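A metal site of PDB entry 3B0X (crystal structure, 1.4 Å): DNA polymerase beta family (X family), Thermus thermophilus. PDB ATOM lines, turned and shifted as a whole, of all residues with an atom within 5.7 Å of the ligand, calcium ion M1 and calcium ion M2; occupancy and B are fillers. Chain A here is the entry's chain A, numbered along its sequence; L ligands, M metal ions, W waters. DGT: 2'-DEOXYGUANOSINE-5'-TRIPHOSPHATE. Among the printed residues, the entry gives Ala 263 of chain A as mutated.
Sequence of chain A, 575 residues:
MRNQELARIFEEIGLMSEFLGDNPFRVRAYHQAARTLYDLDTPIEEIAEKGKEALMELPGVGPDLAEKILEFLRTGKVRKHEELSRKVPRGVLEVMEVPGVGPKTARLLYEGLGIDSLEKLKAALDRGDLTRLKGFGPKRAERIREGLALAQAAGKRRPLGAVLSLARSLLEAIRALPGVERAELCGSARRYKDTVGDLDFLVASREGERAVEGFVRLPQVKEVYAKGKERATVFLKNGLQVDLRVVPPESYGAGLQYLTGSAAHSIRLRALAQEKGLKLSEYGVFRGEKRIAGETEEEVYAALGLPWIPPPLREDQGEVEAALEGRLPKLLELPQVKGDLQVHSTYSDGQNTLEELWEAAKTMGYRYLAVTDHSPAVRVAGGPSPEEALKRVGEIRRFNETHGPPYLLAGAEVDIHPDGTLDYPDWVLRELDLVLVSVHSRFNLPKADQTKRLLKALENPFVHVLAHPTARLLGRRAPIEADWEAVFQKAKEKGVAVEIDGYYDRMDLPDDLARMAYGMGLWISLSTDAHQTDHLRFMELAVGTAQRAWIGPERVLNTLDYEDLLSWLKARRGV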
ATOM      1  N   MET A   1      -5.228  12.092 -27.316  1.00  0.00           N
ATOM      2  CA  MET A   1      -4.387  11.218 -28.188  1.00  0.00           C
ATOM      3  C   MET A   1      -2.916  11.304 -27.839  1.00  0.00           C
ATOM      4  O   MET A   1      -2.424  12.364 -27.442  1.00  0.00           O
ATOM      5  CB  MET A   1      -4.581  11.585 -29.658  1.00  0.00           C
ATOM      6  CG  MET A   1      -5.744  10.875 -30.297  1.00  0.00           C
ATOM      7  SD  MET A   1      -5.708  11.068 -32.082  1.00  0.00           S
ATOM      8  CE  MET A   1      -6.775  12.493 -32.268  1.00  0.00           C
ATOM      9  N   ARG A 157       7.599  33.670 -25.675  1.00  0.00           N
ATOM     10  CA  ARG A 157       6.290  34.252 -26.023  1.00  0.00           C
ATOM     11  C   ARG A 157       6.482  35.689 -26.472  1.00  0.00           C
ATOM     12  O   ARG A 157       7.437  36.333 -26.056  1.00  0.00           O
ATOM     13  CB  ARG A 157       5.332  34.144 -24.841  1.00  0.00           C
ATOM     14  CG  ARG A 157       5.244  32.711 -24.295  1.00  0.00           C
ATOM     15  CD  ARG A 157       4.238  32.574 -23.173  1.00  0.00           C
ATOM     16  NE  ARG A 157       2.868  32.774 -23.639  1.00  0.00           N
ATOM     17  CZ  ARG A 157       2.130  31.857 -24.241  1.00  0.00           C
ATOM     18  NH1 ARG A 157       2.591  30.631 -24.450  1.00  0.00           N
ATOM     19  NH2 ARG A 157       0.893  32.146 -24.603  1.00  0.00           N
ATOM     20  N   CYS A 186      -6.442  30.819 -35.106  1.00  0.00           N
ATOM     21  CA  CYS A 186      -6.997  30.227 -33.900  1.00  0.00           C
ATOM     22  C   CYS A 186      -6.002  30.310 -32.738  1.00  0.00           C
ATOM     23  O   CYS A 186      -5.338  31.338 -32.563  1.00  0.00           O
ATOM     24  CB  CYS A 186      -7.501  28.805 -34.201  1.00  0.00           C
ATOM     25  SG  CYS A 186      -8.843  28.764 -35.431  1.00  0.00           S
ATOM     26  N   GLY A 187      -5.903  29.254 -31.944  1.00  0.00           N
ATOM     27  CA  GLY A 187      -5.028  29.212 -30.783  1.00  0.00           C
ATOM     28  C   GLY A 187      -5.278  30.355 -29.820  1.00  0.00           C
ATOM     29  O   GLY A 187      -6.350  30.987 -29.789  1.00  0.00           O
ATOM     30  N   SER A 188      -4.259  30.652 -29.020  1.00  0.00           N
ATOM     31  CA  SER A 188      -4.384  31.673 -27.963  1.00  0.00           C
ATOM     32  C   SER A 188      -4.574  33.084 -28.545  1.00  0.00           C
ATOM     33  O   SER A 188      -5.174  33.941 -27.885  1.00  0.00           O
ATOM     34  CB  SER A 188      -3.183  31.627 -27.045  1.00  0.00           C
ATOM     35  OG  SER A 188      -2.009  31.890 -27.792  1.00  0.00           O
ATOM     36  N   ALA A 189      -4.144  33.305 -29.794  1.00  0.00           N
ATOM     37  CA  ALA A 189      -4.362  34.596 -30.429  1.00  0.00           C
ATOM     38  C   ALA A 189      -5.855  34.881 -30.580  1.00  0.00           C
ATOM     39  O   ALA A 189      -6.297  36.004 -30.333  1.00  0.00           O
ATOM     40  CB  ALA A 189      -3.675  34.673 -31.778  1.00  0.00           C
ATOM     41  N   ARG A 191      -8.127  33.898 -28.706  1.00  0.00           N
ATOM     42  CA  ARG A 191      -8.639  34.140 -27.360  1.00  0.00           C
ATOM     43  C   ARG A 191      -8.158  35.485 -26.786  1.00  0.00           C
ATOM     44  O   ARG A 191      -8.493  35.811 -25.647  1.00  0.00           O
ATOM     45  CB  ARG A 191      -8.289  32.999 -26.412  1.00  0.00           C
ATOM     46  CG  ARG A 191      -8.682  31.613 -26.960  1.00  0.00           C
ATOM     47  CD  ARG A 191      -8.770  30.559 -25.867  1.00  0.00           C
ATOM     48  NE  ARG A 191      -7.582  30.505 -25.018  1.00  0.00           N
ATOM     49  CZ  ARG A 191      -6.451  29.856 -25.296  1.00  0.00           C
ATOM     50  NH1 ARG A 191      -6.296  29.139 -26.408  1.00  0.00           N
ATOM     51  NH2 ARG A 191      -5.410  29.948 -24.439  1.00  0.00           N
ATOM     52  N   LYS A 193      -5.266  36.337 -25.725  1.00  0.00           N
ATOM     53  CA  LYS A 193      -4.237  36.219 -24.690  1.00  0.00           C
ATOM     54  C   LYS A 193      -3.135  37.222 -24.962  1.00  0.00           C
ATOM     55  O   LYS A 193      -2.780  37.436 -26.126  1.00  0.00           O
ATOM     56  CB  LYS A 193      -3.694  34.813 -24.704  1.00  0.00           C
ATOM     57  CG  LYS A 193      -2.937  34.452 -23.434  1.00  0.00           C
ATOM     58  CD  LYS A 193      -2.548  32.981 -23.450  1.00  0.00           C
ATOM     59  CE  LYS A 193      -1.708  32.609 -22.243  1.00  0.00           C
ATOM     60  NZ  LYS A 193      -2.611  32.509 -21.050  1.00  0.00           N
ATOM     61  N   THR A 195       0.100  37.419 -24.468  1.00  0.00           N
ATOM     62  CA  THR A 195       1.331  36.935 -25.079  1.00  0.00           C
ATOM     63  C   THR A 195       0.979  35.605 -25.706  1.00  0.00           C
ATOM     64  O   THR A 195       0.090  34.888 -25.222  1.00  0.00           O
ATOM     65  CB  THR A 195       2.504  36.759 -24.098  1.00  0.00           C
ATOM     66  OG1 THR A 195       2.266  35.662 -23.212  1.00  0.00           O
ATOM     67  CG2 THR A 195       2.772  38.056 -23.315  1.00  0.00           C
ATOM     68  N   VAL A 196       1.675  35.267 -26.783  1.00  0.00           N
ATOM     69  CA  VAL A 196       1.380  34.059 -27.543  1.00  0.00           C
ATOM     70  C   VAL A 196       2.639  33.274 -27.812  1.00  0.00           C
ATOM     71  O   VAL A 196       3.723  33.855 -27.975  1.00  0.00           O
ATOM     72  CB  VAL A 196       0.633  34.367 -28.859  1.00  0.00           C
ATOM     73  CG1 VAL A 196      -0.714  35.009 -28.565  1.00  0.00           C
ATOM     74  CG2 VAL A 196       1.489  35.252 -29.776  1.00  0.00           C
ATOM     75  N   GLY A 197       2.480  31.961 -27.904  1.00  0.00           N
ATOM     76  CA  GLY A 197       3.536  31.080 -28.416  1.00  0.00           C
ATOM     77  C   GLY A 197       3.422  31.043 -29.916  1.00  0.00           C
ATOM     78  O   GLY A 197       3.328  32.070 -30.585  1.00  0.00           O
ATOM     79  N   ASP A 198       3.434  29.841 -30.484  1.00  0.00           N
ATOM     80  CA  ASP A 198       3.267  29.729 -31.930  1.00  0.00           C
ATOM     81  C   ASP A 198       1.867  30.177 -32.384  1.00  0.00           C
ATOM     82  O   ASP A 198       0.950  30.326 -31.565  1.00  0.00           O
ATOM     83  CB  ASP A 198       3.619  28.331 -32.447  1.00  0.00           C
ATOM     84  CG  ASP A 198       2.646  27.256 -31.979  1.00  0.00           C
ATOM     85  OD1 ASP A 198       1.534  27.552 -31.489  1.00  0.00           O
ATOM     86  OD2 ASP A 198       2.990  26.068 -32.100  1.00  0.00           O
ATOM     87  N   LEU A 199       1.744  30.461 -33.683  1.00  0.00           N
ATOM     88  CA  LEU A 199       0.447  30.839 -34.255  1.00  0.00           C
ATOM     89  C   LEU A 199      -0.164  29.648 -34.940  1.00  0.00           C
ATOM     90  O   LEU A 199       0.552  28.869 -35.557  1.00  0.00           O
ATOM     91  CB  LEU A 199       0.624  31.968 -35.249  1.00  0.00           C
ATOM     92  CG  LEU A 199       1.099  33.231 -34.513  1.00  0.00           C
ATOM     93  CD1 LEU A 199       1.742  34.131 -35.525  1.00  0.00           C
ATOM     94  CD2 LEU A 199       0.010  33.961 -33.768  1.00  0.00           C
ATOM     95  N   ASP A 200      -1.484  29.485 -34.808  1.00  0.00           N
ATOM     96  CA  ASP A 200      -2.168  28.291 -35.286  1.00  0.00           C
ATOM     97  C   ASP A 200      -3.273  28.701 -36.227  1.00  0.00           C
ATOM     98  O   ASP A 200      -4.115  29.530 -35.847  1.00  0.00           O
ATOM     99  CB  ASP A 200      -2.786  27.559 -34.088  1.00  0.00           C
ATOM    100  CG  ASP A 200      -1.778  27.314 -33.020  1.00  0.00           C
ATOM    101  OD1 ASP A 200      -1.086  26.291 -33.105  1.00  0.00           O
ATOM    102  OD2 ASP A 200      -1.657  28.149 -32.106  1.00  0.00           O
ATOM    103  N   ASP A 243       1.720  26.812 -37.062  1.00  0.00           N
ATOM    104  CA  ASP A 243       1.093  25.540 -37.280  1.00  0.00           C
ATOM    105  C   ASP A 243      -0.148  25.736 -38.151  1.00  0.00           C
ATOM    106  O   ASP A 243      -0.935  26.673 -37.945  1.00  0.00           O
ATOM    107  CB  ASP A 243       0.604  24.953 -35.963  1.00  0.00           C
ATOM    108  CG  ASP A 243       1.708  24.426 -35.094  1.00  0.00           C
ATOM    109  OD1 ASP A 243       2.837  24.174 -35.548  1.00  0.00           O
ATOM    110  OD2 ASP A 243       1.432  24.223 -33.881  1.00  0.00           O
ATOM    111  N   TYR A 258     -11.681  23.107 -31.779  1.00  0.00           N
ATOM    112  CA  TYR A 258     -10.491  22.353 -31.434  1.00  0.00           C
ATOM    113  C   TYR A 258      -9.253  23.256 -31.371  1.00  0.00           C
ATOM    114  O   TYR A 258      -8.487  23.240 -30.396  1.00  0.00           O
ATOM    115  CB  TYR A 258     -10.300  21.211 -32.430  1.00  0.00           C
ATOM    116  CG  TYR A 258      -9.047  20.433 -32.186  1.00  0.00           C
ATOM    117  CD1 TYR A 258      -9.056  19.292 -31.385  1.00  0.00           C
ATOM    118  CD2 TYR A 258      -7.836  20.848 -32.733  1.00  0.00           C
ATOM    119  CE1 TYR A 258      -7.876  18.588 -31.137  1.00  0.00           C
ATOM    120  CE2 TYR A 258      -6.654  20.168 -32.489  1.00  0.00           C
ATOM    121  CZ  TYR A 258      -6.688  19.037 -31.699  1.00  0.00           C
ATOM    122  OH  TYR A 258      -5.525  18.334 -31.448  1.00  0.00           O
ATOM    123  N   LEU A 259      -9.011  23.983 -32.453  1.00  0.00           N
ATOM    124  CA  LEU A 259      -7.758  24.719 -32.554  1.00  0.00           C
ATOM    125  C   LEU A 259      -7.728  26.018 -31.752  1.00  0.00           C
ATOM    126  O   LEU A 259      -6.658  26.621 -31.546  1.00  0.00           O
ATOM    127  CB  LEU A 259      -7.413  24.967 -34.023  1.00  0.00           C
ATOM    128  CG  LEU A 259      -5.943  25.270 -34.313  1.00  0.00           C
ATOM    129  CD1 LEU A 259      -5.034  24.233 -33.762  1.00  0.00           C
ATOM    130  CD2 LEU A 259      -5.733  25.487 -35.798  1.00  0.00           C
ATOM    131  N   THR A 260      -8.893  26.457 -31.285  1.00  0.00           N
ATOM    132  CA  THR A 260      -8.974  27.670 -30.453  1.00  0.00           C
ATOM    133  C   THR A 260      -8.749  27.367 -28.983  1.00  0.00           C
ATOM    134  O   THR A 260      -8.211  28.195 -28.249  1.00  0.00           O
ATOM    135  CB  THR A 260     -10.321  28.383 -30.688  1.00  0.00           C
ATOM    136  OG1 THR A 260     -10.380  28.783 -32.068  1.00  0.00           O
ATOM    137  CG2 THR A 260     -10.494  29.614 -29.821  1.00  0.00           C
ATOM    138  N   GLY A 261      -9.152  26.178 -28.556  1.00  0.00           N
ATOM    139  CA  GLY A 261      -8.994  25.801 -27.158  1.00  0.00           C
ATOM    140  C   GLY A 261      -9.691  26.803 -26.246  1.00  0.00           C
ATOM    141  O   GLY A 261     -10.732  27.342 -26.585  1.00  0.00           O
ATOM    142  N   SER A 262      -9.152  27.076 -25.050  1.00  0.00           N
ATOM    143  CA  SER A 262      -7.983  26.418 -24.495  1.00  0.00           C
ATOM    144  C   SER A 262      -8.191  24.910 -24.353  1.00  0.00           C
ATOM    145  O   SER A 262      -9.330  24.397 -24.428  1.00  0.00           O
ATOM    146  CB  SER A 262      -7.712  27.003 -23.130  1.00  0.00           C
ATOM    147  OG  SER A 262      -8.688  26.557 -22.193  1.00  0.00           O
ATOM    148  N   ALA A 263      -7.115  24.181 -24.113  1.00  0.00           N
ATOM    149  CA  ALA A 263      -7.225  22.741 -23.880  1.00  0.00           C
ATOM    150  C   ALA A 263      -8.178  22.450 -22.728  1.00  0.00           C
ATOM    151  O   ALA A 263      -8.967  21.492 -22.810  1.00  0.00           O
ATOM    152  CB  ALA A 263      -5.847  22.116 -23.625  1.00  0.00           C
ATOM    153  N   SER A 266     -11.736  22.712 -23.935  1.00  0.00           N
ATOM    154  CA  SER A 266     -12.109  21.562 -24.746  1.00  0.00           C
ATOM    155  C   SER A 266     -12.350  20.301 -23.913  1.00  0.00           C
ATOM    156  O   SER A 266     -13.245  19.508 -24.221  1.00  0.00           O
ATOM    157  CB  SER A 266     -11.071  21.269 -25.816  1.00  0.00           C
ATOM    158  OG  SER A 266     -10.972  22.380 -26.658  1.00  0.00           O
ATOM    159  N   ARG A 270     -15.771  18.135 -24.287  1.00  0.00           N
ATOM    160  CA  ARG A 270     -15.790  16.713 -24.643  1.00  0.00           C
ATOM    161  C   ARG A 270     -16.584  15.877 -23.626  1.00  0.00           C
ATOM    162  O   ARG A 270     -17.268  14.904 -24.000  1.00  0.00           O
ATOM    163  CB  ARG A 270     -14.386  16.140 -24.810  1.00  0.00           C
ATOM    164  CG  ARG A 270     -13.689  16.616 -26.078  1.00  0.00           C
ATOM    165  CD  ARG A 270     -12.495  15.725 -26.417  1.00  0.00           C
ATOM    166  NE  ARG A 270     -11.545  15.712 -25.323  1.00  0.00           N
ATOM    167  CZ  ARG A 270     -10.605  16.632 -25.117  1.00  0.00           C
ATOM    168  NH1 ARG A 270     -10.456  17.645 -25.949  1.00  0.00           N
ATOM    169  NH2 ARG A 270      -9.819  16.514 -24.054  1.00  0.00           N
HETATM  170  PG  DGT L   1       0.207  29.188 -26.895  1.00  0.00           P
HETATM  171  O1G DGT L   1       0.646  28.675 -28.247  1.00  0.00           O
HETATM  172  O2G DGT L   1       0.998  28.672 -25.713  1.00  0.00           O
HETATM  173  O3G DGT L   1       0.085  30.709 -26.829  1.00  0.00           O
HETATM  174  O3B DGT L   1      -1.315  28.694 -26.624  1.00  0.00           O
HETATM  175  PB  DGT L   1      -2.295  27.920 -27.620  1.00  0.00           P
HETATM  176  O1B DGT L   1      -3.616  27.802 -26.937  1.00  0.00           O
HETATM  177  O2B DGT L   1      -2.257  28.502 -28.996  1.00  0.00           O
HETATM  178  O3A DGT L   1      -1.654  26.443 -27.636  1.00  0.00           O
HETATM  179  PA  DGT L   1      -1.059  25.459 -28.756  1.00  0.00           P
HETATM  180  O1A DGT L   1      -0.480  26.228 -29.894  1.00  0.00           O
HETATM  181  O2A DGT L   1      -0.173  24.482 -28.021  1.00  0.00           O
HETATM  182  O5' DGT L   1      -2.310  24.610 -29.227  1.00  0.00           O
HETATM  183  C5' DGT L   1      -3.331  25.256 -30.023  1.00  0.00           C
HETATM  184  C4' DGT L   1      -4.700  24.724 -29.651  1.00  0.00           C
HETATM  185  O4' DGT L   1      -4.742  23.336 -29.950  1.00  0.00           O
HETATM  186  C3' DGT L   1      -5.076  24.803 -28.194  1.00  0.00           C
HETATM  187  O3' DGT L   1      -5.593  26.069 -27.814  1.00  0.00           O
HETATM  188  C2' DGT L   1      -6.119  23.727 -28.053  1.00  0.00           C
HETATM  189  C1' DGT L   1      -5.627  22.676 -29.040  1.00  0.00           C
HETATM  190  N9  DGT L   1      -4.869  21.625 -28.353  1.00  0.00           N
HETATM  191  C8  DGT L   1      -3.562  21.686 -27.986  1.00  0.00           C
HETATM  192  N7  DGT L   1      -3.210  20.529 -27.376  1.00  0.00           N
HETATM  193  C5  DGT L   1      -4.297  19.737 -27.376  1.00  0.00           C
HETATM  194  C6  DGT L   1      -4.609  18.383 -26.888  1.00  0.00           C
HETATM  195  O6  DGT L   1      -3.733  17.684 -26.335  1.00  0.00           O
HETATM  196  N1  DGT L   1      -5.852  17.946 -27.083  1.00  0.00           N
HETATM  197  C2  DGT L   1      -6.814  18.687 -27.684  1.00  0.00           C
HETATM  198  N2  DGT L   1      -8.035  18.160 -27.822  1.00  0.00           N
HETATM  199  N3  DGT L   1      -6.632  19.944 -28.146  1.00  0.00           N
HETATM  200  C4  DGT L   1      -5.384  20.474 -28.027  1.00  0.00           C
HETATM  201 CA    CA M   1       0.652  25.234 -31.879  1.00  0.00          CA
HETATM  202 CA    CA M   2      -0.292  28.606 -30.352  1.00  0.00          CA
HETATM  203  O   HOH W   1      -8.231  19.265 -24.509  1.00  0.00           O
HETATM  204  O   HOH W   2      -8.381  15.208 -27.992  1.00  0.00           O
HETATM  205  O   HOH W   3     -11.020  18.017 -28.742  1.00  0.00           O
HETATM  206  O   HOH W   4      -6.602  15.422 -25.955  1.00  0.00           O
HETATM  207  O   HOH W   5      -3.573  27.810 -24.244  1.00  0.00           O
HETATM  208  O   HOH W   6      -0.172  21.736 -28.369  1.00  0.00           O
HETATM  209  O   HOH W   7      -0.101  24.299 -25.382  1.00  0.00           O
HETATM  210  O   HOH W   8       3.150  27.587 -28.608  1.00  0.00           O
HETATM  211  O   HOH W   9      -0.740  23.325 -31.767  1.00  0.00           O
HETATM  212  O   HOH W  10       1.797  24.031 -30.251  1.00  0.00           O
HETATM  213  O   HOH W  11      -0.662  28.761 -23.393  1.00  0.00           O
HETATM  214  O   HOH W  12      -8.794  21.867 -28.093  1.00  0.00           O
HETATM  215  O   HOH W  13      -1.261  30.956 -30.267  1.00  0.00           O
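Within 4 Å of calcium ion M1: Asp 198, Asp 200 and Asp 243. The nearest printed residue that does not touch calcium ion M1 is Leu 199 (5.2 Å).
Water W10 is bound to calcium ion M1 (2.3 Å). Calcium ion M1 is bound by water W9. OD2 of Asp 243 binds calcium ion M1 (2.4 Å). Calcium ion M1 is bound by the side-chain carboxylate (OD1) of Asp 200, at 2.4 Å. Calcium ion M1 is bound by O1A of the ligand (2.5 Å). Calcium ion M1 is bound by OD2 of Asp 198 (2.5 Å). The side-chain carboxylate (OD1) of Asp 198 is bound to calcium ion M1, 2.5 Å away.
O of Asp 200 lies within hydrogen-bond range of N of Cys 186, at 2.8 Å. The backbone carbonyl oxygen (O) of Ser 188 is in hydrogen-bond range of the backbone NH (N) of Lys 193 (3.2 Å). The backbone carbonyl oxygen of Leu 259 lies within hydrogen-bond range of the backbone NH of Gly 187. The backbone carbonyl oxygen of Leu 199 lies within hydrogen-bond range of the backbone NH of Asp 243 (2.8 Å). The side-chain hydroxyl (OG1) of Thr 260 lies close to the side-chain sulfur (SG) of Cys 186. NH2 of Arg 157 lies within hydrogen-bond range of O of Thr 195 (2.9 Å). The guanidinium group of Arg 191 lies within hydrogen-bond range of the backbone carbonyl oxygen of Thr 260 (2.8 Å).
NH1 of Arg 270 sits close to N2 of the ligand (3.1 Å). Gly 187 touches the ligand. Val 196 touches the ligand. O of Tyr 258 touches C1' of the ligand (3.2 Å). Leu 259 touches the ligand. CA of Gly 261 touches O3' of the ligand, 3.5 Å away. The nearest printed residue that does not touch the ligand is Ala 263 (4.1 Å).
The nearest printed residue that does not touch calcium ion M2 is Leu 199 (4.3 Å).
Water W5 bridges an oxygen (O1B) of the ligand (2.7 Å) and the guanidinium group (NH2) of Arg 191 (2.8 Å). Water W12 lies within hydrogen-bond range of the side-chain hydroxyl (OG) of Ser 266 (2.7 Å), the backbone carbonyl oxygen (O) of Tyr 258 (2.7 Å) and a nitrogen (N3) of the ligand (2.9 Å). Water W3 bridges the guanidinium group (NH1) of Arg 270 (2.9 Å) and a nitrogen (N2) of the ligand (3.1 Å). Water W1 lies within hydrogen-bond range of the backbone carbonyl oxygen (O) of Ala 263, the guanidinium group (NH1) of Arg 270 and a nitrogen (N2) of the ligand.
O of Thr 260 is in hydrogen-bond range of O3' of the ligand, at 3.4 Å. The guanidinium group (NH1) of Arg 191 is in salt-bridge range of an oxygen (O1B) of the ligand, 3.0 Å away. N of Ser 188 lies close to O2B of the ligand (2.9 Å). The side-chain hydroxyl of Ser 188 is in hydrogen-bond range of an oxygen (O3G) of the ligand. O3G of the ligand lies within hydrogen-bond range of N of Gly 197 (2.9 Å). NH2 of Arg 157 is in salt-bridge range of O3G of the ligand (2.8 Å).
OD2 of Asp 200 binds calcium ion M2, at 2.3 Å. Calcium ion M2 is bound by O1G of the ligand (2.3 Å). Calcium ion M2 is bound by O2B of the ligand (2.4 Å). The side-chain carboxylate (OD1) of Asp 198 binds calcium ion M2 (2.4 Å). Calcium ion M2 is bound by O1A of the ligand (2.4 Å). The backbone carbonyl oxygen (O) of Asp 198 binds calcium ion M2 (2.4 Å). Water W13 is bound to calcium ion M2 (2.5 Å). Calcium ion M2 has seven donor atoms within binding distance.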
